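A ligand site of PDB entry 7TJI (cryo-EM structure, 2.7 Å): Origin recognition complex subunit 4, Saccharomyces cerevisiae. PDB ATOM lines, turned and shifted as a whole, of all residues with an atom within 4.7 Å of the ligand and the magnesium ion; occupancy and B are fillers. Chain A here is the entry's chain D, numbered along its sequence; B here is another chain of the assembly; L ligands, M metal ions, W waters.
Residues that only touch the magnesium ion: Lys 151 of chain B (3.9 Å) and Glu 154 of chain B (3.9 Å).
Within 4 Å of the magnesium ion: Thr 112, Lys 151 of chain B and Glu 154 of chain B.
The guanidinium group (NH1) of Arg 107 is in salt-bridge range of the side-chain carboxylate (OE2) of Glu 221 (2.7 Å).
The backbone carbonyl oxygen of Pro 106 is in hydrogen-bond range of the side-chain amino group of Lys 111.
The side-chain amino group (NZ) of Lys 151 of chain B lies within salt-bridge range of the side-chain carboxylate (OE2) of Glu 154 of chain B, at 3.9 Å.
The side-chain hydroxyl (OG) of Ser 109 is in hydrogen-bond range of the backbone carbonyl oxygen (O) of Pro 106 (2.7 Å).
The side-chain amide nitrogen of Gln 108 sits close to the backbone carbonyl oxygen of His 182 of chain B, at 3.5 Å.
The magnesium ion is bound by OG1 of Thr 112 (2.0 Å), O2 of the ligand (2.1 Å), water W3 (2.1 Å), water W1 (2.2 Å), water W4 (2.3 Å) and O4 of the ligand (2.6 Å).
The magnesium ion has six donor atoms within binding distance.
The backbone carbonyl oxygen of Pro 106 sits close to an oxygen (O5) of the ligand (3.4 Å).
NZ of Lys 158 of chain B lies close to N3 of the ligand (3.4 Å).
Tyr 64 touches the ligand (O to N5, 3.8 Å).
Gly 65 touches the ligand (O to C9, 3.4 Å).
Hydrophobic or aromatic side chains within 4 Å of the ligand: Tyr 110 and Tyr 113.
Within 4 Å of the ligand: Tyr 64, Gly 65, Pro 106, Arg 107, Gln 108, Ser 109, Tyr 110, Lys 111, Thr 112, Tyr 113, Asp 116, Lys 341, Lys 151 of chain B and Lys 158 of chain B.
Water W3 lies within hydrogen-bond range of the side-chain carboxylate of Glu 154 of chain B (2.6 Å), the side-chain amino group of Lys 151 of chain B (2.8 Å) and an oxygen (O7) of the ligand (3.1 Å).
Water W1 lies within hydrogen-bond range of OE1 of Glu 154 of chain B (2.6 Å) and OD2 of Asp 220 (3.3 Å).
Water W2 lies within hydrogen-bond range of O3 of the ligand (2.4 Å), NE2 of Gln 108 (2.6 Å) and ND1 of His 182 of chain B (2.9 Å).
Water W6 bridges OE2 of Glu 221 (3.1 Å) and O1 of the ligand (3.1 Å).
Water W5 bridges the backbone carbonyl oxygen (O) of Tyr 113 (3.1 Å) and a nitrogen (N3) of the ligand (3.5 Å).
An oxygen (O8) of the ligand is in hydrogen-bond range of the backbone NH (N) of Tyr 113 (2.7 Å).
NZ of Lys 151 of chain B lies within salt-bridge range of O3 of the ligand (3.3 Å).
NZ of Lys 341 sits at hydrogen-bond distance from O12 of the ligand, 2.8 Å away.
The side-chain carboxylate (OD2) of Asp 116 lies within hydrogen-bond range of a nitrogen (N3) of the ligand (3.2 Å).
N of Gln 108 sits at hydrogen-bond distance from O6 of the ligand, at 3.4 Å.
The backbone NH (N) of Lys 111 is in hydrogen-bond range of an oxygen (O5) of the ligand.
NZ of Lys 111 is in salt-bridge range of O1 of the ligand, 2.5 Å away.
O8 of the ligand sits at hydrogen-bond distance from N of Thr 112, at 2.9 Å.
An oxygen (O5) of the ligand sits at hydrogen-bond distance from the backbone NH (N) of Tyr 110 (3.4 Å).
O5 of the ligand is in hydrogen-bond range of N of Ser 109 (3.0 Å).
O3 of the ligand is in salt-bridge range of NH1 of Arg 107, 3.0 Å away.
OG of Ser 109 sits at hydrogen-bond distance from O5 of the ligand, at 3.5 Å.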
ATOM      1  N   TYR A  64      -9.597 -11.661  -4.134  1.00  0.00           N
ATOM      2  CA  TYR A  64      -9.807 -11.903  -2.720  1.00  0.00           C
ATOM      3  C   TYR A  64      -8.919 -11.045  -1.825  1.00  0.00           C
ATOM      4  O   TYR A  64      -9.057 -11.104  -0.606  1.00  0.00           O
ATOM      5  CB  TYR A  64      -9.582 -13.389  -2.381  1.00  0.00           C
ATOM      6  CG  TYR A  64     -10.764 -14.273  -2.694  1.00  0.00           C
ATOM      7  CD1 TYR A  64     -11.871 -14.328  -1.857  1.00  0.00           C
ATOM      8  CD2 TYR A  64     -10.767 -15.056  -3.832  1.00  0.00           C
ATOM      9  CE1 TYR A  64     -12.947 -15.140  -2.146  1.00  0.00           C
ATOM     10  CE2 TYR A  64     -11.835 -15.866  -4.133  1.00  0.00           C
ATOM     11  CZ  TYR A  64     -12.911 -15.910  -3.291  1.00  0.00           C
ATOM     12  OH  TYR A  64     -13.968 -16.731  -3.621  1.00  0.00           O
ATOM     13  N   GLY A  65      -8.024 -10.262  -2.412  1.00  0.00           N
ATOM     14  CA  GLY A  65      -7.182  -9.366  -1.639  1.00  0.00           C
ATOM     15  C   GLY A  65      -6.158 -10.046  -0.770  1.00  0.00           C
ATOM     16  O   GLY A  65      -5.690  -9.453   0.202  1.00  0.00           O
ATOM     17  N   PRO A 106     -20.413   2.421   5.967  1.00  0.00           N
ATOM     18  CA  PRO A 106     -21.304   1.263   5.776  1.00  0.00           C
ATOM     19  C   PRO A 106     -20.552  -0.056   5.829  1.00  0.00           C
ATOM     20  O   PRO A 106     -19.320  -0.126   5.919  1.00  0.00           O
ATOM     21  CB  PRO A 106     -21.900   1.499   4.380  1.00  0.00           C
ATOM     22  CG  PRO A 106     -21.080   2.547   3.761  1.00  0.00           C
ATOM     23  CD  PRO A 106     -20.516   3.379   4.855  1.00  0.00           C
ATOM     24  N   ARG A 107     -21.325  -1.134   5.816  1.00  0.00           N
ATOM     25  CA  ARG A 107     -20.751  -2.466   5.729  1.00  0.00           C
ATOM     26  C   ARG A 107     -20.062  -2.651   4.387  1.00  0.00           C
ATOM     27  O   ARG A 107     -20.503  -2.109   3.370  1.00  0.00           O
ATOM     28  CB  ARG A 107     -21.819  -3.533   5.932  1.00  0.00           C
ATOM     29  CG  ARG A 107     -22.500  -3.470   7.269  1.00  0.00           C
ATOM     30  CD  ARG A 107     -22.892  -4.843   7.754  1.00  0.00           C
ATOM     31  NE  ARG A 107     -23.369  -4.809   9.137  1.00  0.00           N
ATOM     32  CZ  ARG A 107     -22.587  -4.848  10.200  1.00  0.00           C
ATOM     33  NH1 ARG A 107     -21.269  -4.942  10.092  1.00  0.00           N
ATOM     34  NH2 ARG A 107     -23.129  -4.801  11.417  1.00  0.00           N
ATOM     35  N   GLN A 108     -18.959  -3.401   4.414  1.00  0.00           N
ATOM     36  CA  GLN A 108     -18.097  -3.680   3.254  1.00  0.00           C
ATOM     37  C   GLN A 108     -17.546  -2.401   2.628  1.00  0.00           C
ATOM     38  O   GLN A 108     -17.414  -2.296   1.406  1.00  0.00           O
ATOM     39  CB  GLN A 108     -18.822  -4.533   2.198  1.00  0.00           C
ATOM     40  CG  GLN A 108     -19.354  -5.856   2.742  1.00  0.00           C
ATOM     41  CD  GLN A 108     -18.256  -6.770   3.257  1.00  0.00           C
ATOM     42  OE1 GLN A 108     -17.495  -7.334   2.481  1.00  0.00           O
ATOM     43  NE2 GLN A 108     -18.169  -6.908   4.566  1.00  0.00           N
ATOM     44  N   SER A 109     -17.207  -1.429   3.466  1.00  0.00           N
ATOM     45  CA  SER A 109     -16.632  -0.165   3.021  1.00  0.00           C
ATOM     46  C   SER A 109     -15.169  -0.021   3.448  1.00  0.00           C
ATOM     47  O   SER A 109     -14.694   1.101   3.658  1.00  0.00           O
ATOM     48  CB  SER A 109     -17.454   1.022   3.524  1.00  0.00           C
ATOM     49  OG  SER A 109     -17.258   1.249   4.906  1.00  0.00           O
ATOM     50  N   TYR A 110     -14.484  -1.160   3.610  1.00  0.00           N
ATOM     51  CA  TYR A 110     -13.035  -1.267   3.778  1.00  0.00           C
ATOM     52  C   TYR A 110     -12.530  -0.665   5.090  1.00  0.00           C
ATOM     53  O   TYR A 110     -11.392  -0.213   5.168  1.00  0.00           O
ATOM     54  CB  TYR A 110     -12.276  -0.665   2.595  1.00  0.00           C
ATOM     55  CG  TYR A 110     -12.586  -1.339   1.280  1.00  0.00           C
ATOM     56  CD1 TYR A 110     -11.896  -2.470   0.885  1.00  0.00           C
ATOM     57  CD2 TYR A 110     -13.594  -0.853   0.446  1.00  0.00           C
ATOM     58  CE1 TYR A 110     -12.183  -3.110  -0.306  1.00  0.00           C
ATOM     59  CE2 TYR A 110     -13.886  -1.482  -0.738  1.00  0.00           C
ATOM     60  CZ  TYR A 110     -13.172  -2.605  -1.116  1.00  0.00           C
ATOM     61  OH  TYR A 110     -13.465  -3.233  -2.299  1.00  0.00           O
ATOM     62  N   LYS A 111     -13.353  -0.686   6.148  1.00  0.00           N
ATOM     63  CA  LYS A 111     -12.865  -0.261   7.461  1.00  0.00           C
ATOM     64  C   LYS A 111     -11.899  -1.283   8.039  1.00  0.00           C
ATOM     65  O   LYS A 111     -10.819  -0.915   8.522  1.00  0.00           O
ATOM     66  CB  LYS A 111     -14.041  -0.035   8.420  1.00  0.00           C
ATOM     67  CG  LYS A 111     -15.088   0.927   7.897  1.00  0.00           C
ATOM     68  CD  LYS A 111     -16.097   1.318   8.972  1.00  0.00           C
ATOM     69  CE  LYS A 111     -16.826   0.101   9.509  1.00  0.00           C
ATOM     70  NZ  LYS A 111     -17.774  -0.481   8.526  1.00  0.00           N
ATOM     71  N   THR A 112     -12.257  -2.570   7.995  1.00  0.00           N
ATOM     72  CA  THR A 112     -11.370  -3.618   8.491  1.00  0.00           C
ATOM     73  C   THR A 112     -10.178  -3.801   7.561  1.00  0.00           C
ATOM     74  O   THR A 112      -9.057  -4.052   8.025  1.00  0.00           O
ATOM     75  CB  THR A 112     -12.157  -4.916   8.659  1.00  0.00           C
ATOM     76  OG1 THR A 112     -13.221  -4.703   9.592  1.00  0.00           O
ATOM     77  CG2 THR A 112     -11.293  -6.056   9.163  1.00  0.00           C
ATOM     78  N   TYR A 113     -10.399  -3.649   6.247  1.00  0.00           N
ATOM     79  CA  TYR A 113      -9.348  -3.848   5.258  1.00  0.00           C
ATOM     80  C   TYR A 113      -8.212  -2.845   5.424  1.00  0.00           C
ATOM     81  O   TYR A 113      -7.035  -3.220   5.419  1.00  0.00           O
ATOM     82  CB  TYR A 113      -9.956  -3.763   3.855  1.00  0.00           C
ATOM     83  CG  TYR A 113      -8.978  -3.914   2.712  1.00  0.00           C
ATOM     84  CD1 TYR A 113      -8.568  -5.163   2.267  1.00  0.00           C
ATOM     85  CD2 TYR A 113      -8.483  -2.789   2.041  1.00  0.00           C
ATOM     86  CE1 TYR A 113      -7.686  -5.298   1.220  1.00  0.00           C
ATOM     87  CE2 TYR A 113      -7.600  -2.924   0.994  1.00  0.00           C
ATOM     88  CZ  TYR A 113      -7.205  -4.175   0.582  1.00  0.00           C
ATOM     89  OH  TYR A 113      -6.330  -4.313  -0.454  1.00  0.00           O
ATOM     90  N   ASP A 116      -6.358  -3.494   8.807  1.00  0.00           N
ATOM     91  CA  ASP A 116      -5.498  -4.672   8.695  1.00  0.00           C
ATOM     92  C   ASP A 116      -4.285  -4.380   7.833  1.00  0.00           C
ATOM     93  O   ASP A 116      -3.177  -4.848   8.121  1.00  0.00           O
ATOM     94  CB  ASP A 116      -6.291  -5.847   8.138  1.00  0.00           C
ATOM     95  CG  ASP A 116      -7.073  -6.568   9.211  1.00  0.00           C
ATOM     96  OD1 ASP A 116      -6.730  -6.420  10.397  1.00  0.00           O
ATOM     97  OD2 ASP A 116      -8.035  -7.296   8.868  1.00  0.00           O
ATOM     98  N   ASP A 220     -14.538  -3.386  16.728  1.00  0.00           N
ATOM     99  CA  ASP A 220     -15.568  -3.494  15.705  1.00  0.00           C
ATOM    100  C   ASP A 220     -16.946  -3.520  16.344  1.00  0.00           C
ATOM    101  O   ASP A 220     -17.132  -4.076  17.431  1.00  0.00           O
ATOM    102  CB  ASP A 220     -15.357  -4.768  14.874  1.00  0.00           C
ATOM    103  CG  ASP A 220     -14.093  -4.720  14.049  1.00  0.00           C
ATOM    104  OD1 ASP A 220     -13.844  -3.684  13.391  1.00  0.00           O
ATOM    105  OD2 ASP A 220     -13.343  -5.714  14.037  1.00  0.00           O
ATOM    106  N   GLU A 221     -17.914  -2.906  15.657  1.00  0.00           N
ATOM    107  CA  GLU A 221     -19.300  -2.714  16.118  1.00  0.00           C
ATOM    108  C   GLU A 221     -19.346  -2.024  17.485  1.00  0.00           C
ATOM    109  O   GLU A 221     -19.980  -2.504  18.425  1.00  0.00           O
ATOM    110  CB  GLU A 221     -20.086  -4.030  16.155  1.00  0.00           C
ATOM    111  CG  GLU A 221     -19.925  -4.893  14.925  1.00  0.00           C
ATOM    112  CD  GLU A 221     -20.789  -4.418  13.770  1.00  0.00           C
ATOM    113  OE1 GLU A 221     -21.850  -3.821  14.025  1.00  0.00           O
ATOM    114  OE2 GLU A 221     -20.401  -4.654  12.610  1.00  0.00           O
ATOM    115  N   THR A 255     -21.296   1.385  11.738  1.00  0.00           N
ATOM    116  CA  THR A 255     -22.074   1.824  10.588  1.00  0.00           C
ATOM    117  C   THR A 255     -22.970   3.013  10.908  1.00  0.00           C
ATOM    118  O   THR A 255     -23.538   3.598   9.982  1.00  0.00           O
ATOM    119  CB  THR A 255     -22.925   0.683  10.035  1.00  0.00           C
ATOM    120  OG1 THR A 255     -23.793   0.177  11.051  1.00  0.00           O
ATOM    121  CG2 THR A 255     -22.051  -0.444   9.511  1.00  0.00           C
ATOM    122  N   PRO A 338     -17.435  -5.004  -3.489  1.00  0.00           N
ATOM    123  CA  PRO A 338     -17.578  -6.420  -3.103  1.00  0.00           C
ATOM    124  C   PRO A 338     -18.700  -7.166  -3.816  1.00  0.00           C
ATOM    125  O   PRO A 338     -18.529  -8.355  -4.125  1.00  0.00           O
ATOM    126  CB  PRO A 338     -17.837  -6.345  -1.591  1.00  0.00           C
ATOM    127  CG  PRO A 338     -17.109  -5.163  -1.166  1.00  0.00           C
ATOM    128  CD  PRO A 338     -17.235  -4.170  -2.276  1.00  0.00           C
ATOM    129  N   LYS A 341     -17.260  -7.997  -7.133  1.00  0.00           N
ATOM    130  CA  LYS A 341     -16.229  -9.011  -6.981  1.00  0.00           C
ATOM    131  C   LYS A 341     -16.846 -10.400  -6.819  1.00  0.00           C
ATOM    132  O   LYS A 341     -16.298 -11.389  -7.340  1.00  0.00           O
ATOM    133  CB  LYS A 341     -15.352  -8.691  -5.769  1.00  0.00           C
ATOM    134  CG  LYS A 341     -14.290  -7.655  -6.025  1.00  0.00           C
ATOM    135  CD  LYS A 341     -13.271  -7.617  -4.897  1.00  0.00           C
ATOM    136  CE  LYS A 341     -13.932  -7.362  -3.556  1.00  0.00           C
ATOM    137  NZ  LYS A 341     -12.979  -6.833  -2.547  1.00  0.00           N
ATOM    138  N   LYS B 151     -18.573 -12.764  11.601  1.00  0.00           N
ATOM    139  CA  LYS B 151     -17.367 -12.084  12.046  1.00  0.00           C
ATOM    140  C   LYS B 151     -16.409 -12.967  12.854  1.00  0.00           C
ATOM    141  O   LYS B 151     -15.424 -12.455  13.385  1.00  0.00           O
ATOM    142  CB  LYS B 151     -17.743 -10.846  12.867  1.00  0.00           C
ATOM    143  CG  LYS B 151     -18.410  -9.737  12.055  1.00  0.00           C
ATOM    144  CD  LYS B 151     -17.598  -9.360  10.830  1.00  0.00           C
ATOM    145  CE  LYS B 151     -18.216  -8.186  10.089  1.00  0.00           C
ATOM    146  NZ  LYS B 151     -17.643  -8.004   8.730  1.00  0.00           N
ATOM    147  N   GLU B 154     -12.496 -13.151  11.845  1.00  0.00           N
ATOM    148  CA  GLU B 154     -11.656 -12.006  12.136  1.00  0.00           C
ATOM    149  C   GLU B 154     -11.016 -12.072  13.521  1.00  0.00           C
ATOM    150  O   GLU B 154     -10.078 -11.306  13.782  1.00  0.00           O
ATOM    151  CB  GLU B 154     -12.466 -10.724  12.004  1.00  0.00           C
ATOM    152  CG  GLU B 154     -12.941 -10.455  10.590  1.00  0.00           C
ATOM    153  CD  GLU B 154     -13.736  -9.170  10.476  1.00  0.00           C
ATOM    154  OE1 GLU B 154     -14.201  -8.664  11.521  1.00  0.00           O
ATOM    155  OE2 GLU B 154     -13.898  -8.662   9.356  1.00  0.00           O
ATOM    156  N   LYS B 158      -4.335 -14.851  11.929  1.00  0.00           N
ATOM    157  CA  LYS B 158      -4.297 -14.641  10.485  1.00  0.00           C
ATOM    158  C   LYS B 158      -3.335 -15.583   9.785  1.00  0.00           C
ATOM    159  O   LYS B 158      -3.614 -16.023   8.660  1.00  0.00           O
ATOM    160  CB  LYS B 158      -3.944 -13.186  10.198  1.00  0.00           C
ATOM    161  CG  LYS B 158      -5.142 -12.327   9.863  1.00  0.00           C
ATOM    162  CD  LYS B 158      -5.790 -12.765   8.565  1.00  0.00           C
ATOM    163  CE  LYS B 158      -6.666 -11.680   7.973  1.00  0.00           C
ATOM    164  NZ  LYS B 158      -6.974 -11.925   6.542  1.00  0.00           N
ATOM    165  N   HIS B 182     -23.675  -7.599   3.984  1.00  0.00           N
ATOM    166  CA  HIS B 182     -22.415  -8.268   4.289  1.00  0.00           C
ATOM    167  C   HIS B 182     -21.712  -8.786   3.044  1.00  0.00           C
ATOM    168  O   HIS B 182     -20.507  -9.044   3.117  1.00  0.00           O
ATOM    169  CB  HIS B 182     -22.659  -9.426   5.265  1.00  0.00           C
ATOM    170  CG  HIS B 182     -22.884  -8.983   6.676  1.00  0.00           C
ATOM    171  ND1 HIS B 182     -21.860  -8.563   7.493  1.00  0.00           N
ATOM    172  CD2 HIS B 182     -24.021  -8.873   7.404  1.00  0.00           C
ATOM    173  CE1 HIS B 182     -22.345  -8.230   8.673  1.00  0.00           C
ATOM    174  NE2 HIS B 182     -23.655  -8.402   8.650  1.00  0.00           N
HETATM  175  P1  LIG L   1     -18.154  -4.121   8.446  1.00  0.00           P
HETATM  176  O1  LIG L   1     -18.771  -2.813   8.773  1.00  0.00           O
HETATM  177  O2  LIG L   1     -17.311  -4.675   9.552  1.00  0.00           O
HETATM  178  O3  LIG L   1     -19.146  -5.180   8.035  1.00  0.00           O
HETATM  179  P2  LIG L   1     -15.921  -3.168   6.740  1.00  0.00           P
HETATM  180  O4  LIG L   1     -14.891  -3.183   7.779  1.00  0.00           O
HETATM  181  O5  LIG L   1     -16.392  -1.803   6.288  1.00  0.00           O
HETATM  182  O6  LIG L   1     -17.177  -3.983   7.196  1.00  0.00           O
HETATM  183  P3  LIG L   1     -14.223  -4.785   4.985  1.00  0.00           P
HETATM  184  O7  LIG L   1     -14.389  -6.208   5.312  1.00  0.00           O
HETATM  185  O8  LIG L   1     -13.009  -4.121   5.601  1.00  0.00           O
HETATM  186  O9  LIG L   1     -15.476  -3.964   5.449  1.00  0.00           O
HETATM  187  O10 LIG L   1     -14.108  -4.493   3.438  1.00  0.00           O
HETATM  188  C1  LIG L   1     -14.869  -5.238   2.469  1.00  0.00           C
HETATM  189  C2  LIG L   1     -13.970  -5.981   1.526  1.00  0.00           C
HETATM  190  O11 LIG L   1     -12.633  -6.076   2.085  1.00  0.00           O
HETATM  191  C3  LIG L   1     -14.409  -7.414   1.228  1.00  0.00           C
HETATM  192  O12 LIG L   1     -14.185  -7.744  -0.133  1.00  0.00           O
HETATM  193  C4  LIG L   1     -13.545  -8.240   2.194  1.00  0.00           C
HETATM  194  O13 LIG L   1     -13.351  -9.564   1.724  1.00  0.00           O
HETATM  195  C5  LIG L   1     -12.248  -7.438   2.136  1.00  0.00           C
HETATM  196  N1  LIG L   1     -11.355  -7.629   3.278  1.00  0.00           N
HETATM  197  C6  LIG L   1     -11.607  -7.333   4.588  1.00  0.00           C
HETATM  198  N2  LIG L   1     -10.614  -7.608   5.392  1.00  0.00           N
HETATM  199  C7  LIG L   1      -9.629  -8.124   4.554  1.00  0.00           C
HETATM  200  C8  LIG L   1      -8.331  -8.603   4.791  1.00  0.00           C
HETATM  201  N3  LIG L   1      -7.755  -8.646   5.996  1.00  0.00           N
HETATM  202  N4  LIG L   1      -7.624  -9.038   3.719  1.00  0.00           N
HETATM  203  C9  LIG L   1      -8.186  -8.998   2.514  1.00  0.00           C
HETATM  204  N5  LIG L   1      -9.403  -8.572   2.173  1.00  0.00           N
HETATM  205  C10 LIG L   1     -10.082  -8.142   3.244  1.00  0.00           C
HETATM  206 MG    MG M   1     -15.241  -4.998   9.604  1.00  0.00          MG
HETATM  207  O   HOH W   1     -15.314  -6.299  11.404  1.00  0.00           O
HETATM  208  O   HOH W   2     -20.059  -6.662   6.364  1.00  0.00           O
HETATM  209  O   HOH W   3     -15.260  -6.662   8.278  1.00  0.00           O
HETATM  210  O   HOH W   4     -15.310  -2.979  10.623  1.00  0.00           O
HETATM  211  O   HOH W   5      -6.116  -5.997   4.480  1.00  0.00           O
HETATM  212  O   HOH W   6     -18.984  -1.997  11.798  1.00  0.00           O
HETATM  213  O   HOH W   7     -18.085  -5.607  12.234  1.00  0.00           O
